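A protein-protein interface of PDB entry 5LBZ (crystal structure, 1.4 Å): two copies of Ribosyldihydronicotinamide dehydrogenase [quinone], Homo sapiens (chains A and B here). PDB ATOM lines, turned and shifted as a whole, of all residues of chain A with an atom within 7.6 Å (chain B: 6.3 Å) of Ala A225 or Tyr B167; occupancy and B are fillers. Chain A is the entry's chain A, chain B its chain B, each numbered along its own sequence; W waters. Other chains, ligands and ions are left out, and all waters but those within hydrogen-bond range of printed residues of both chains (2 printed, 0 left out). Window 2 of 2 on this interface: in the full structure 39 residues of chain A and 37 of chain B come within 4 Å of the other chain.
Of the printed residues of chain B, Tyr A167 touches Trp B170 (3.5 Å) and Phe B229 (3.5 Å).
Ala A225 touches just one residue of chain B: Tyr B167 (3.8 Å).
Printed residues of chain B within 4 Å of Phe A229: Tyr B167 (3.5 Å) and Phe B229 (3.2 Å).
Lys B158 touches none of the printed residues of chain A.
Printed residues of chain A within 4 Å of Asn B162: Trp A170.
Of chain A, only Trp A170, Ala A225 and Phe A229 come within 4 Å of Tyr B167.
Of the printed residues of chain A, Trp B170 touches Tyr A167.
The nearest residue of chain B that does not touch Ala A225 is Lys B158 (5.6 Å).
Of the 15 printed residues of chain B, 4 touch a printed residue of chain A.
Printed residues of chain A that touch a printed residue of chain B: Tyr A167, Trp A170, Ala A225 and Phe A229.
Among the printed residues, 7 pairs touch across the chains.
Among the printed residues, no Asp or Glu carboxylate lies within 4 Å of a Lys or Arg side-chain nitrogen of the other chain.
Among the printed residues, merely in contact across the chains: Tyr A167 with Trp B170, Tyr A167 with Phe B229, Trp A170 with Asn B162, Trp A170 with Tyr B167, Ala A225 with Tyr B167, Phe A229 with Tyr B167 and Phe A229 with Phe B229.
Water W2 bridges the backbone carbonyl oxygen (O) of Tyr A167 and the backbone carbonyl oxygen (O) of Tyr B167.
Water W1 lies within hydrogen-bond range of O of Asn B162 (2.8 Å), O of Asp B164 (2.8 Å) and NE1 of Trp A170 (2.9 Å).
Tyr A167 touches Trp B170, and with the chains exchanged Trp A170 touches Tyr B167.
Tyr A167 touches Phe B229, and with the chains exchanged Phe A229 touches Tyr B167.
Phe B229 touches its own counterpart, Phe A229.
7 positions are printed for both chains.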
ATOM      1  N   TYR A 167     -28.111  -6.342  17.425  1.00  0.00           N
ATOM      2  CA  TYR A 167     -27.606  -5.491  16.373  1.00  0.00           C
ATOM      3  C   TYR A 167     -26.437  -6.135  15.621  1.00  0.00           C
ATOM      4  O   TYR A 167     -26.377  -6.029  14.415  1.00  0.00           O
ATOM      5  CB  TYR A 167     -27.170  -4.123  16.891  1.00  0.00           C
ATOM      6  CG  TYR A 167     -28.165  -3.244  17.551  1.00  0.00           C
ATOM      7  CD1 TYR A 167     -29.541  -3.432  17.470  1.00  0.00           C
ATOM      8  CD2 TYR A 167     -27.722  -2.139  18.246  1.00  0.00           C
ATOM      9  CE1 TYR A 167     -30.424  -2.535  18.086  1.00  0.00           C
ATOM     10  CE2 TYR A 167     -28.593  -1.214  18.812  1.00  0.00           C
ATOM     11  CZ  TYR A 167     -29.954  -1.429  18.730  1.00  0.00           C
ATOM     12  OH  TYR A 167     -30.837  -0.558  19.308  1.00  0.00           O
ATOM     13  N   PHE A 168     -25.528  -6.772  16.343  1.00  0.00           N
ATOM     14  CA  PHE A 168     -24.391  -7.377  15.705  1.00  0.00           C
ATOM     15  C   PHE A 168     -24.699  -8.689  15.013  1.00  0.00           C
ATOM     16  O   PHE A 168     -23.898  -9.191  14.225  1.00  0.00           O
ATOM     17  CB  PHE A 168     -23.150  -7.459  16.638  1.00  0.00           C
ATOM     18  CG  PHE A 168     -23.228  -8.462  17.769  1.00  0.00           C
ATOM     19  CD1 PHE A 168     -23.227  -9.830  17.546  1.00  0.00           C
ATOM     20  CD2 PHE A 168     -23.279  -8.037  19.102  1.00  0.00           C
ATOM     21  CE1 PHE A 168     -23.308 -10.759  18.569  1.00  0.00           C
ATOM     22  CE2 PHE A 168     -23.356  -8.951  20.136  1.00  0.00           C
ATOM     23  CZ  PHE A 168     -23.348 -10.316  19.880  1.00  0.00           C
ATOM     24  N   TRP A 170     -26.963  -9.265  12.803  1.00  0.00           N
ATOM     25  CA  TRP A 170     -27.543  -9.079  11.457  1.00  0.00           C
ATOM     26  C   TRP A 170     -26.719  -9.659  10.300  1.00  0.00           C
ATOM     27  O   TRP A 170     -27.277 -10.385   9.480  1.00  0.00           O
ATOM     28  CB  TRP A 170     -27.842  -7.601  11.259  1.00  0.00           C
ATOM     29  CG  TRP A 170     -28.281  -7.202   9.911  1.00  0.00           C
ATOM     30  CD1 TRP A 170     -27.572  -6.511   8.992  1.00  0.00           C
ATOM     31  CD2 TRP A 170     -29.608  -7.321   9.389  1.00  0.00           C
ATOM     32  NE1 TRP A 170     -28.360  -6.263   7.871  1.00  0.00           N
ATOM     33  CE2 TRP A 170     -29.613  -6.773   8.097  1.00  0.00           C
ATOM     34  CE3 TRP A 170     -30.760  -7.920   9.851  1.00  0.00           C
ATOM     35  CZ2 TRP A 170     -30.752  -6.746   7.307  1.00  0.00           C
ATOM     36  CZ3 TRP A 170     -31.879  -7.910   9.047  1.00  0.00           C
ATOM     37  CH2 TRP A 170     -31.861  -7.320   7.790  1.00  0.00           C
ATOM     38  N   PRO A 171     -25.412  -9.348  10.205  1.00  0.00           N
ATOM     39  CA  PRO A 171     -24.676  -9.925   9.083  1.00  0.00           C
ATOM     40  C   PRO A 171     -24.634 -11.440   9.065  1.00  0.00           C
ATOM     41  O   PRO A 171     -24.593 -12.038   8.018  1.00  0.00           O
ATOM     42  CB  PRO A 171     -23.270  -9.343   9.242  1.00  0.00           C
ATOM     43  CG  PRO A 171     -23.456  -8.107  10.063  1.00  0.00           C
ATOM     44  CD  PRO A 171     -24.585  -8.439  11.014  1.00  0.00           C
ATOM     45  N   HIS A 174     -29.007 -12.716   9.115  1.00  0.00           N
ATOM     46  CA  HIS A 174     -29.690 -12.332   7.891  1.00  0.00           C
ATOM     47  C   HIS A 174     -28.826 -12.480   6.676  1.00  0.00           C
ATOM     48  O   HIS A 174     -29.198 -13.175   5.717  1.00  0.00           O
ATOM     49  CB  HIS A 174     -30.257 -10.928   7.996  1.00  0.00           C
ATOM     50  CG  HIS A 174     -31.052 -10.504   6.809  1.00  0.00           C
ATOM     51  ND1 HIS A 174     -32.343 -10.921   6.633  1.00  0.00           N
ATOM     52  CD2 HIS A 174     -30.736  -9.759   5.741  1.00  0.00           C
ATOM     53  CE1 HIS A 174     -32.806 -10.376   5.523  1.00  0.00           C
ATOM     54  NE2 HIS A 174     -31.844  -9.696   4.955  1.00  0.00           N
ATOM     55  N   PRO A 222     -37.924 -14.822  13.590  1.00  0.00           N
ATOM     56  CA  PRO A 222     -38.143 -14.171  12.321  1.00  0.00           C
ATOM     57  C   PRO A 222     -36.917 -13.375  12.016  1.00  0.00           C
ATOM     58  O   PRO A 222     -36.566 -12.437  12.721  1.00  0.00           O
ATOM     59  CB  PRO A 222     -39.331 -13.242  12.577  1.00  0.00           C
ATOM     60  CG  PRO A 222     -39.332 -13.015  14.029  1.00  0.00           C
ATOM     61  CD  PRO A 222     -38.755 -14.256  14.648  1.00  0.00           C
ATOM     62  N   CYS A 223     -36.267 -13.727  10.941  1.00  0.00           N
ATOM     63  CA  CYS A 223     -35.020 -13.119  10.634  1.00  0.00           C
ATOM     64  C   CYS A 223     -35.204 -11.867   9.804  1.00  0.00           C
ATOM     65  O   CYS A 223     -35.049 -11.904   8.568  1.00  0.00           O
ATOM     66  CB  CYS A 223     -34.151 -14.165   9.953  1.00  0.00           C
ATOM     67  SG  CYS A 223     -32.519 -13.534   9.760  1.00  0.00           S
ATOM     68  N   THR A 224     -35.653 -10.803  10.488  1.00  0.00           N
ATOM     69  CA  THR A 224     -36.055  -9.538   9.868  1.00  0.00           C
ATOM     70  C   THR A 224     -35.324  -8.373  10.454  1.00  0.00           C
ATOM     71  O   THR A 224     -34.764  -8.462  11.549  1.00  0.00           O
ATOM     72  CB  THR A 224     -37.560  -9.288  10.102  1.00  0.00           C
ATOM     73  OG1 THR A 224     -37.790  -9.234  11.516  1.00  0.00           O
ATOM     74  CG2 THR A 224     -38.380 -10.363   9.475  1.00  0.00           C
ATOM     75  N   ALA A 225     -35.320  -7.258   9.742  1.00  0.00           N
ATOM     76  CA  ALA A 225     -34.748  -6.049  10.315  1.00  0.00           C
ATOM     77  C   ALA A 225     -35.476  -5.682  11.590  1.00  0.00           C
ATOM     78  O   ALA A 225     -34.881  -5.249  12.564  1.00  0.00           O
ATOM     79  CB  ALA A 225     -34.760  -4.915   9.311  1.00  0.00           C
ATOM     80  N   HIS A 226     -36.798  -5.879  11.600  1.00  0.00           N
ATOM     81  CA  HIS A 226     -37.522  -5.563  12.813  1.00  0.00           C
ATOM     82  C   HIS A 226     -37.068  -6.365  14.037  1.00  0.00           C
ATOM     83  O   HIS A 226     -36.897  -5.832  15.133  1.00  0.00           O
ATOM     84  CB  HIS A 226     -38.998  -5.800  12.552  1.00  0.00           C
ATOM     85  CG  HIS A 226     -39.850  -5.490  13.721  1.00  0.00           C
ATOM     86  ND1 HIS A 226     -40.104  -4.203  14.141  1.00  0.00           N
ATOM     87  CD2 HIS A 226     -40.492  -6.304  14.583  1.00  0.00           C
ATOM     88  CE1 HIS A 226     -40.896  -4.240  15.194  1.00  0.00           C
ATOM     89  NE2 HIS A 226     -41.134  -5.509  15.482  1.00  0.00           N
ATOM     90  N   TRP A 227     -36.858  -7.660  13.862  1.00  0.00           N
ATOM     91  CA  TRP A 227     -36.352  -8.465  14.954  1.00  0.00           C
ATOM     92  C   TRP A 227     -35.005  -7.937  15.463  1.00  0.00           C
ATOM     93  O   TRP A 227     -34.760  -7.866  16.651  1.00  0.00           O
ATOM     94  CB  TRP A 227     -36.248  -9.931  14.552  1.00  0.00           C
ATOM     95  CG  TRP A 227     -35.880 -10.862  15.687  1.00  0.00           C
ATOM     96  CD1 TRP A 227     -36.735 -11.552  16.501  1.00  0.00           C
ATOM     97  CD2 TRP A 227     -34.571 -11.199  16.129  1.00  0.00           C
ATOM     98  NE1 TRP A 227     -36.047 -12.293  17.393  1.00  0.00           N
ATOM     99  CE2 TRP A 227     -34.710 -12.091  17.201  1.00  0.00           C
ATOM    100  CE3 TRP A 227     -33.288 -10.826  15.735  1.00  0.00           C
ATOM    101  CZ2 TRP A 227     -33.621 -12.596  17.891  1.00  0.00           C
ATOM    102  CZ3 TRP A 227     -32.205 -11.351  16.389  1.00  0.00           C
ATOM    103  CH2 TRP A 227     -32.366 -12.241  17.468  1.00  0.00           C
ATOM    104  N   HIS A 228     -34.120  -7.600  14.544  1.00  0.00           N
ATOM    105  CA  HIS A 228     -32.779  -7.220  14.930  1.00  0.00           C
ATOM    106  C   HIS A 228     -32.693  -5.806  15.508  1.00  0.00           C
ATOM    107  O   HIS A 228     -31.927  -5.615  16.462  1.00  0.00           O
ATOM    108  CB  HIS A 228     -31.845  -7.326  13.729  1.00  0.00           C
ATOM    109  CG  HIS A 228     -31.512  -8.730  13.337  1.00  0.00           C
ATOM    110  ND1 HIS A 228     -32.300  -9.504  12.512  1.00  0.00           N
ATOM    111  CD2 HIS A 228     -30.476  -9.528  13.707  1.00  0.00           C
ATOM    112  CE1 HIS A 228     -31.751 -10.702  12.366  1.00  0.00           C
ATOM    113  NE2 HIS A 228     -30.631 -10.737  13.064  1.00  0.00           N
ATOM    114  N   PHE A 229     -33.458  -4.867  14.958  1.00  0.00           N
ATOM    115  CA  PHE A 229     -33.273  -3.469  15.291  1.00  0.00           C
ATOM    116  C   PHE A 229     -34.450  -2.770  15.964  1.00  0.00           C
ATOM    117  O   PHE A 229     -34.278  -1.660  16.434  1.00  0.00           O
ATOM    118  CB  PHE A 229     -32.889  -2.696  14.017  1.00  0.00           C
ATOM    119  CG  PHE A 229     -31.749  -3.323  13.247  1.00  0.00           C
ATOM    120  CD1 PHE A 229     -30.529  -3.573  13.852  1.00  0.00           C
ATOM    121  CD2 PHE A 229     -31.925  -3.739  11.947  1.00  0.00           C
ATOM    122  CE1 PHE A 229     -29.532  -4.188  13.148  1.00  0.00           C
ATOM    123  CE2 PHE A 229     -30.918  -4.357  11.259  1.00  0.00           C
ATOM    124  CZ  PHE A 229     -29.731  -4.601  11.856  1.00  0.00           C
ATOM    125  N   GLY A 230     -35.628  -3.376  15.927  1.00  0.00           N
ATOM    126  CA  GLY A 230     -36.892  -2.700  16.359  1.00  0.00           C
ATOM    127  C   GLY A 230     -36.988  -2.526  17.860  1.00  0.00           C
ATOM    128  O   GLY A 230     -36.344  -3.254  18.614  1.00  0.00           O
ATOM    129  N   THR B 157     -31.535  -1.276   0.694  1.00  0.00           N
ATOM    130  CA  THR B 157     -32.442  -0.259   1.276  1.00  0.00           C
ATOM    131  C   THR B 157     -33.291  -0.928   2.315  1.00  0.00           C
ATOM    132  O   THR B 157     -33.411  -2.174   2.356  1.00  0.00           O
ATOM    133  CB  THR B 157     -33.336   0.399   0.246  1.00  0.00           C
ATOM    134  OG1 THR B 157     -34.109  -0.594  -0.447  1.00  0.00           O
ATOM    135  CG2 THR B 157     -32.479   1.239  -0.705  1.00  0.00           C
ATOM    136  N   LYS B 158     -33.928  -0.127   3.149  1.00  0.00           N
ATOM    137  CA  LYS B 158     -34.743  -0.675   4.219  1.00  0.00           C
ATOM    138  C   LYS B 158     -35.813  -1.632   3.711  1.00  0.00           C
ATOM    139  O   LYS B 158     -36.091  -2.640   4.360  1.00  0.00           O
ATOM    140  CB  LYS B 158     -35.376   0.465   5.026  1.00  0.00           C
ATOM    141  CG  LYS B 158     -36.118   0.000   6.245  1.00  0.00           C
ATOM    142  CD  LYS B 158     -36.623   1.193   7.059  1.00  0.00           C
ATOM    143  CE  LYS B 158     -37.478   0.743   8.239  1.00  0.00           C
ATOM    144  NZ  LYS B 158     -38.628  -0.118   7.809  1.00  0.00           N
ATOM    145  N   ASN B 162     -31.965  -6.881   1.220  1.00  0.00           N
ATOM    146  CA  ASN B 162     -30.791  -6.904   2.101  1.00  0.00           C
ATOM    147  C   ASN B 162     -30.836  -5.964   3.258  1.00  0.00           C
ATOM    148  O   ASN B 162     -29.939  -6.025   4.120  1.00  0.00           O
ATOM    149  CB  ASN B 162     -29.539  -6.602   1.287  1.00  0.00           C
ATOM    150  CG  ASN B 162     -29.211  -7.679   0.266  1.00  0.00           C
ATOM    151  OD1 ASN B 162     -29.545  -8.822   0.413  1.00  0.00           O
ATOM    152  ND2 ASN B 162     -28.506  -7.270  -0.791  1.00  0.00           N
ATOM    153  N   GLY B 163     -31.878  -5.133   3.355  1.00  0.00           N
ATOM    154  CA  GLY B 163     -31.902  -4.083   4.367  1.00  0.00           C
ATOM    155  C   GLY B 163     -30.938  -2.955   4.044  1.00  0.00           C
ATOM    156  O   GLY B 163     -30.156  -3.041   3.102  1.00  0.00           O
ATOM    157  N   ASP B 164     -31.014  -1.861   4.786  1.00  0.00           N
ATOM    158  CA  ASP B 164     -30.163  -0.677   4.523  1.00  0.00           C
ATOM    159  C   ASP B 164     -28.686  -1.090   4.616  1.00  0.00           C
ATOM    160  O   ASP B 164     -28.294  -1.848   5.501  1.00  0.00           O
ATOM    161  CB  ASP B 164     -30.479   0.405   5.566  1.00  0.00           C
ATOM    162  CG  ASP B 164     -29.784   1.777   5.338  1.00  0.00           C
ATOM    163  OD1 ASP B 164     -28.856   1.983   4.553  1.00  0.00           O
ATOM    164  OD2 ASP B 164     -30.234   2.737   5.970  1.00  0.00           O
ATOM    165  N   SER B 165     -27.868  -0.539   3.729  1.00  0.00           N
ATOM    166  CA  SER B 165     -26.429  -0.779   3.819  1.00  0.00           C
ATOM    167  C   SER B 165     -25.870  -0.377   5.171  1.00  0.00           C
ATOM    168  O   SER B 165     -24.927  -1.008   5.688  1.00  0.00           O
ATOM    169  CB  SER B 165     -25.684  -0.026   2.722  1.00  0.00           C
ATOM    170  OG  SER B 165     -25.930   1.369   2.798  1.00  0.00           O
ATOM    171  N   ARG B 166     -26.440   0.647   5.793  1.00  0.00           N
ATOM    172  CA  ARG B 166     -25.914   1.076   7.072  1.00  0.00           C
ATOM    173  C   ARG B 166     -26.017  -0.027   8.136  1.00  0.00           C
ATOM    174  O   ARG B 166     -25.222  -0.073   9.068  1.00  0.00           O
ATOM    175  CB  ARG B 166     -26.615   2.332   7.558  1.00  0.00           C
ATOM    176  CG  ARG B 166     -26.380   3.556   6.700  1.00  0.00           C
ATOM    177  CD  ARG B 166     -26.892   4.798   7.394  1.00  0.00           C
ATOM    178  NE  ARG B 166     -26.727   5.994   6.581  1.00  0.00           N
ATOM    179  CZ  ARG B 166     -26.949   7.222   7.026  1.00  0.00           C
ATOM    180  NH1 ARG B 166     -27.372   7.412   8.247  1.00  0.00           N
ATOM    181  NH2 ARG B 166     -26.750   8.247   6.203  1.00  0.00           N
ATOM    182  N   TYR B 167     -26.991  -0.918   7.989  1.00  0.00           N
ATOM    183  CA  TYR B 167     -27.196  -1.950   8.984  1.00  0.00           C
ATOM    184  C   TYR B 167     -25.969  -2.838   9.146  1.00  0.00           C
ATOM    185  O   TYR B 167     -25.633  -3.210  10.254  1.00  0.00           O
ATOM    186  CB  TYR B 167     -28.389  -2.850   8.658  1.00  0.00           C
ATOM    187  CG  TYR B 167     -29.741  -2.222   8.609  1.00  0.00           C
ATOM    188  CD1 TYR B 167     -30.037  -0.959   9.098  1.00  0.00           C
ATOM    189  CD2 TYR B 167     -30.785  -2.956   8.074  1.00  0.00           C
ATOM    190  CE1 TYR B 167     -31.330  -0.459   9.048  1.00  0.00           C
ATOM    191  CE2 TYR B 167     -32.085  -2.469   8.046  1.00  0.00           C
ATOM    192  CZ  TYR B 167     -32.351  -1.211   8.518  1.00  0.00           C
ATOM    193  OH  TYR B 167     -33.629  -0.709   8.450  1.00  0.00           O
ATOM    194  N   PHE B 168     -25.339  -3.237   8.033  1.00  0.00           N
ATOM    195  CA  PHE B 168     -24.181  -4.127   8.126  1.00  0.00           C
ATOM    196  C   PHE B 168     -22.919  -3.423   8.574  1.00  0.00           C
ATOM    197  O   PHE B 168     -21.942  -4.075   8.919  1.00  0.00           O
ATOM    198  CB  PHE B 168     -23.995  -4.966   6.846  1.00  0.00           C
ATOM    199  CG  PHE B 168     -23.544  -4.199   5.598  1.00  0.00           C
ATOM    200  CD1 PHE B 168     -22.270  -3.657   5.491  1.00  0.00           C
ATOM    201  CD2 PHE B 168     -24.384  -4.063   4.494  1.00  0.00           C
ATOM    202  CE1 PHE B 168     -21.872  -2.945   4.366  1.00  0.00           C
ATOM    203  CE2 PHE B 168     -23.970  -3.376   3.358  1.00  0.00           C
ATOM    204  CZ  PHE B 168     -22.702  -2.824   3.280  1.00  0.00           C
ATOM    205  N   LEU B 169     -22.921  -2.091   8.561  1.00  0.00           N
ATOM    206  CA  LEU B 169     -21.739  -1.353   8.969  1.00  0.00           C
ATOM    207  C   LEU B 169     -21.508  -1.346  10.472  1.00  0.00           C
ATOM    208  O   LEU B 169     -20.399  -1.042  10.921  1.00  0.00           O
ATOM    209  CB  LEU B 169     -21.797   0.072   8.424  1.00  0.00           C
ATOM    210  CG  LEU B 169     -21.728   0.204   6.920  1.00  0.00           C
ATOM    211  CD1 LEU B 169     -21.963   1.673   6.532  1.00  0.00           C
ATOM    212  CD2 LEU B 169     -20.436  -0.286   6.358  1.00  0.00           C
ATOM    213  N   TRP B 170     -22.517  -1.684  11.269  1.00  0.00           N
ATOM    214  CA  TRP B 170     -22.429  -1.551  12.718  1.00  0.00           C
ATOM    215  C   TRP B 170     -21.247  -2.292  13.360  1.00  0.00           C
ATOM    216  O   TRP B 170     -20.512  -1.677  14.143  1.00  0.00           O
ATOM    217  CB  TRP B 170     -23.771  -1.972  13.315  1.00  0.00           C
ATOM    218  CG  TRP B 170     -23.805  -2.029  14.801  1.00  0.00           C
ATOM    219  CD1 TRP B 170     -23.830  -3.145  15.584  1.00  0.00           C
ATOM    220  CD2 TRP B 170     -23.980  -0.906  15.695  1.00  0.00           C
ATOM    221  NE1 TRP B 170     -23.951  -2.772  16.908  1.00  0.00           N
ATOM    222  CE2 TRP B 170     -24.045  -1.412  17.000  1.00  0.00           C
ATOM    223  CE3 TRP B 170     -24.056   0.454  15.508  1.00  0.00           C
ATOM    224  CZ2 TRP B 170     -24.217  -0.583  18.106  1.00  0.00           C
ATOM    225  CZ3 TRP B 170     -24.243   1.272  16.575  1.00  0.00           C
ATOM    226  CH2 TRP B 170     -24.302   0.756  17.858  1.00  0.00           C
ATOM    227  N   PRO B 171     -21.028  -3.578  13.073  1.00  0.00           N
ATOM    228  CA  PRO B 171     -19.895  -4.228  13.700  1.00  0.00           C
ATOM    229  C   PRO B 171     -18.544  -3.606  13.386  1.00  0.00           C
ATOM    230  O   PRO B 171     -17.638  -3.615  14.208  1.00  0.00           O
ATOM    231  CB  PRO B 171     -19.955  -5.653  13.154  1.00  0.00           C
ATOM    232  CG  PRO B 171     -21.364  -5.840  12.735  1.00  0.00           C
ATOM    233  CD  PRO B 171     -21.810  -4.504  12.229  1.00  0.00           C
ATOM    234  N   HIS B 228     -26.988   4.304  12.255  1.00  0.00           N
ATOM    235  CA  HIS B 228     -26.994   3.006  11.583  1.00  0.00           C
ATOM    236  C   HIS B 228     -28.397   2.481  11.303  1.00  0.00           C
ATOM    237  O   HIS B 228     -28.618   1.905  10.245  1.00  0.00           O
ATOM    238  CB  HIS B 228     -26.200   1.992  12.399  1.00  0.00           C
ATOM    239  CG  HIS B 228     -24.715   2.218  12.362  1.00  0.00           C
ATOM    240  ND1 HIS B 228     -24.058   3.080  13.220  1.00  0.00           N
ATOM    241  CD2 HIS B 228     -23.770   1.713  11.547  1.00  0.00           C
ATOM    242  CE1 HIS B 228     -22.766   3.085  12.932  1.00  0.00           C
ATOM    243  NE2 HIS B 228     -22.562   2.248  11.932  1.00  0.00           N
ATOM    244  N   PHE B 229     -29.323   2.667  12.237  1.00  0.00           N
ATOM    245  CA  PHE B 229     -30.608   1.955  12.189  1.00  0.00           C
ATOM    246  C   PHE B 229     -31.839   2.842  12.018  1.00  0.00           C
ATOM    247  O   PHE B 229     -32.890   2.336  11.717  1.00  0.00           O
ATOM    248  CB  PHE B 229     -30.767   1.049  13.405  1.00  0.00           C
ATOM    249  CG  PHE B 229     -29.552   0.189  13.669  1.00  0.00           C
ATOM    250  CD1 PHE B 229     -29.046  -0.672  12.715  1.00  0.00           C
ATOM    251  CD2 PHE B 229     -28.907   0.264  14.889  1.00  0.00           C
ATOM    252  CE1 PHE B 229     -27.890  -1.393  12.947  1.00  0.00           C
ATOM    253  CE2 PHE B 229     -27.756  -0.474  15.112  1.00  0.00           C
ATOM    254  CZ  PHE B 229     -27.267  -1.303  14.163  1.00  0.00           C
ATOM    255  N   GLY B 230     -31.683   4.144  12.219  1.00  0.00           N
ATOM    256  CA  GLY B 230     -32.808   5.114  12.098  1.00  0.00           C
ATOM    257  C   GLY B 230     -33.213   5.361  10.660  1.00  0.00           C
ATOM    258  O   GLY B 230     -32.443   5.111   9.731  1.00  0.00           O
HETATM  259  O   HOH W   1     -27.934  -4.653   5.480  1.00  0.00           O
HETATM  260  O   HOH W   2     -25.094  -5.252  12.090  1.00  0.00           O
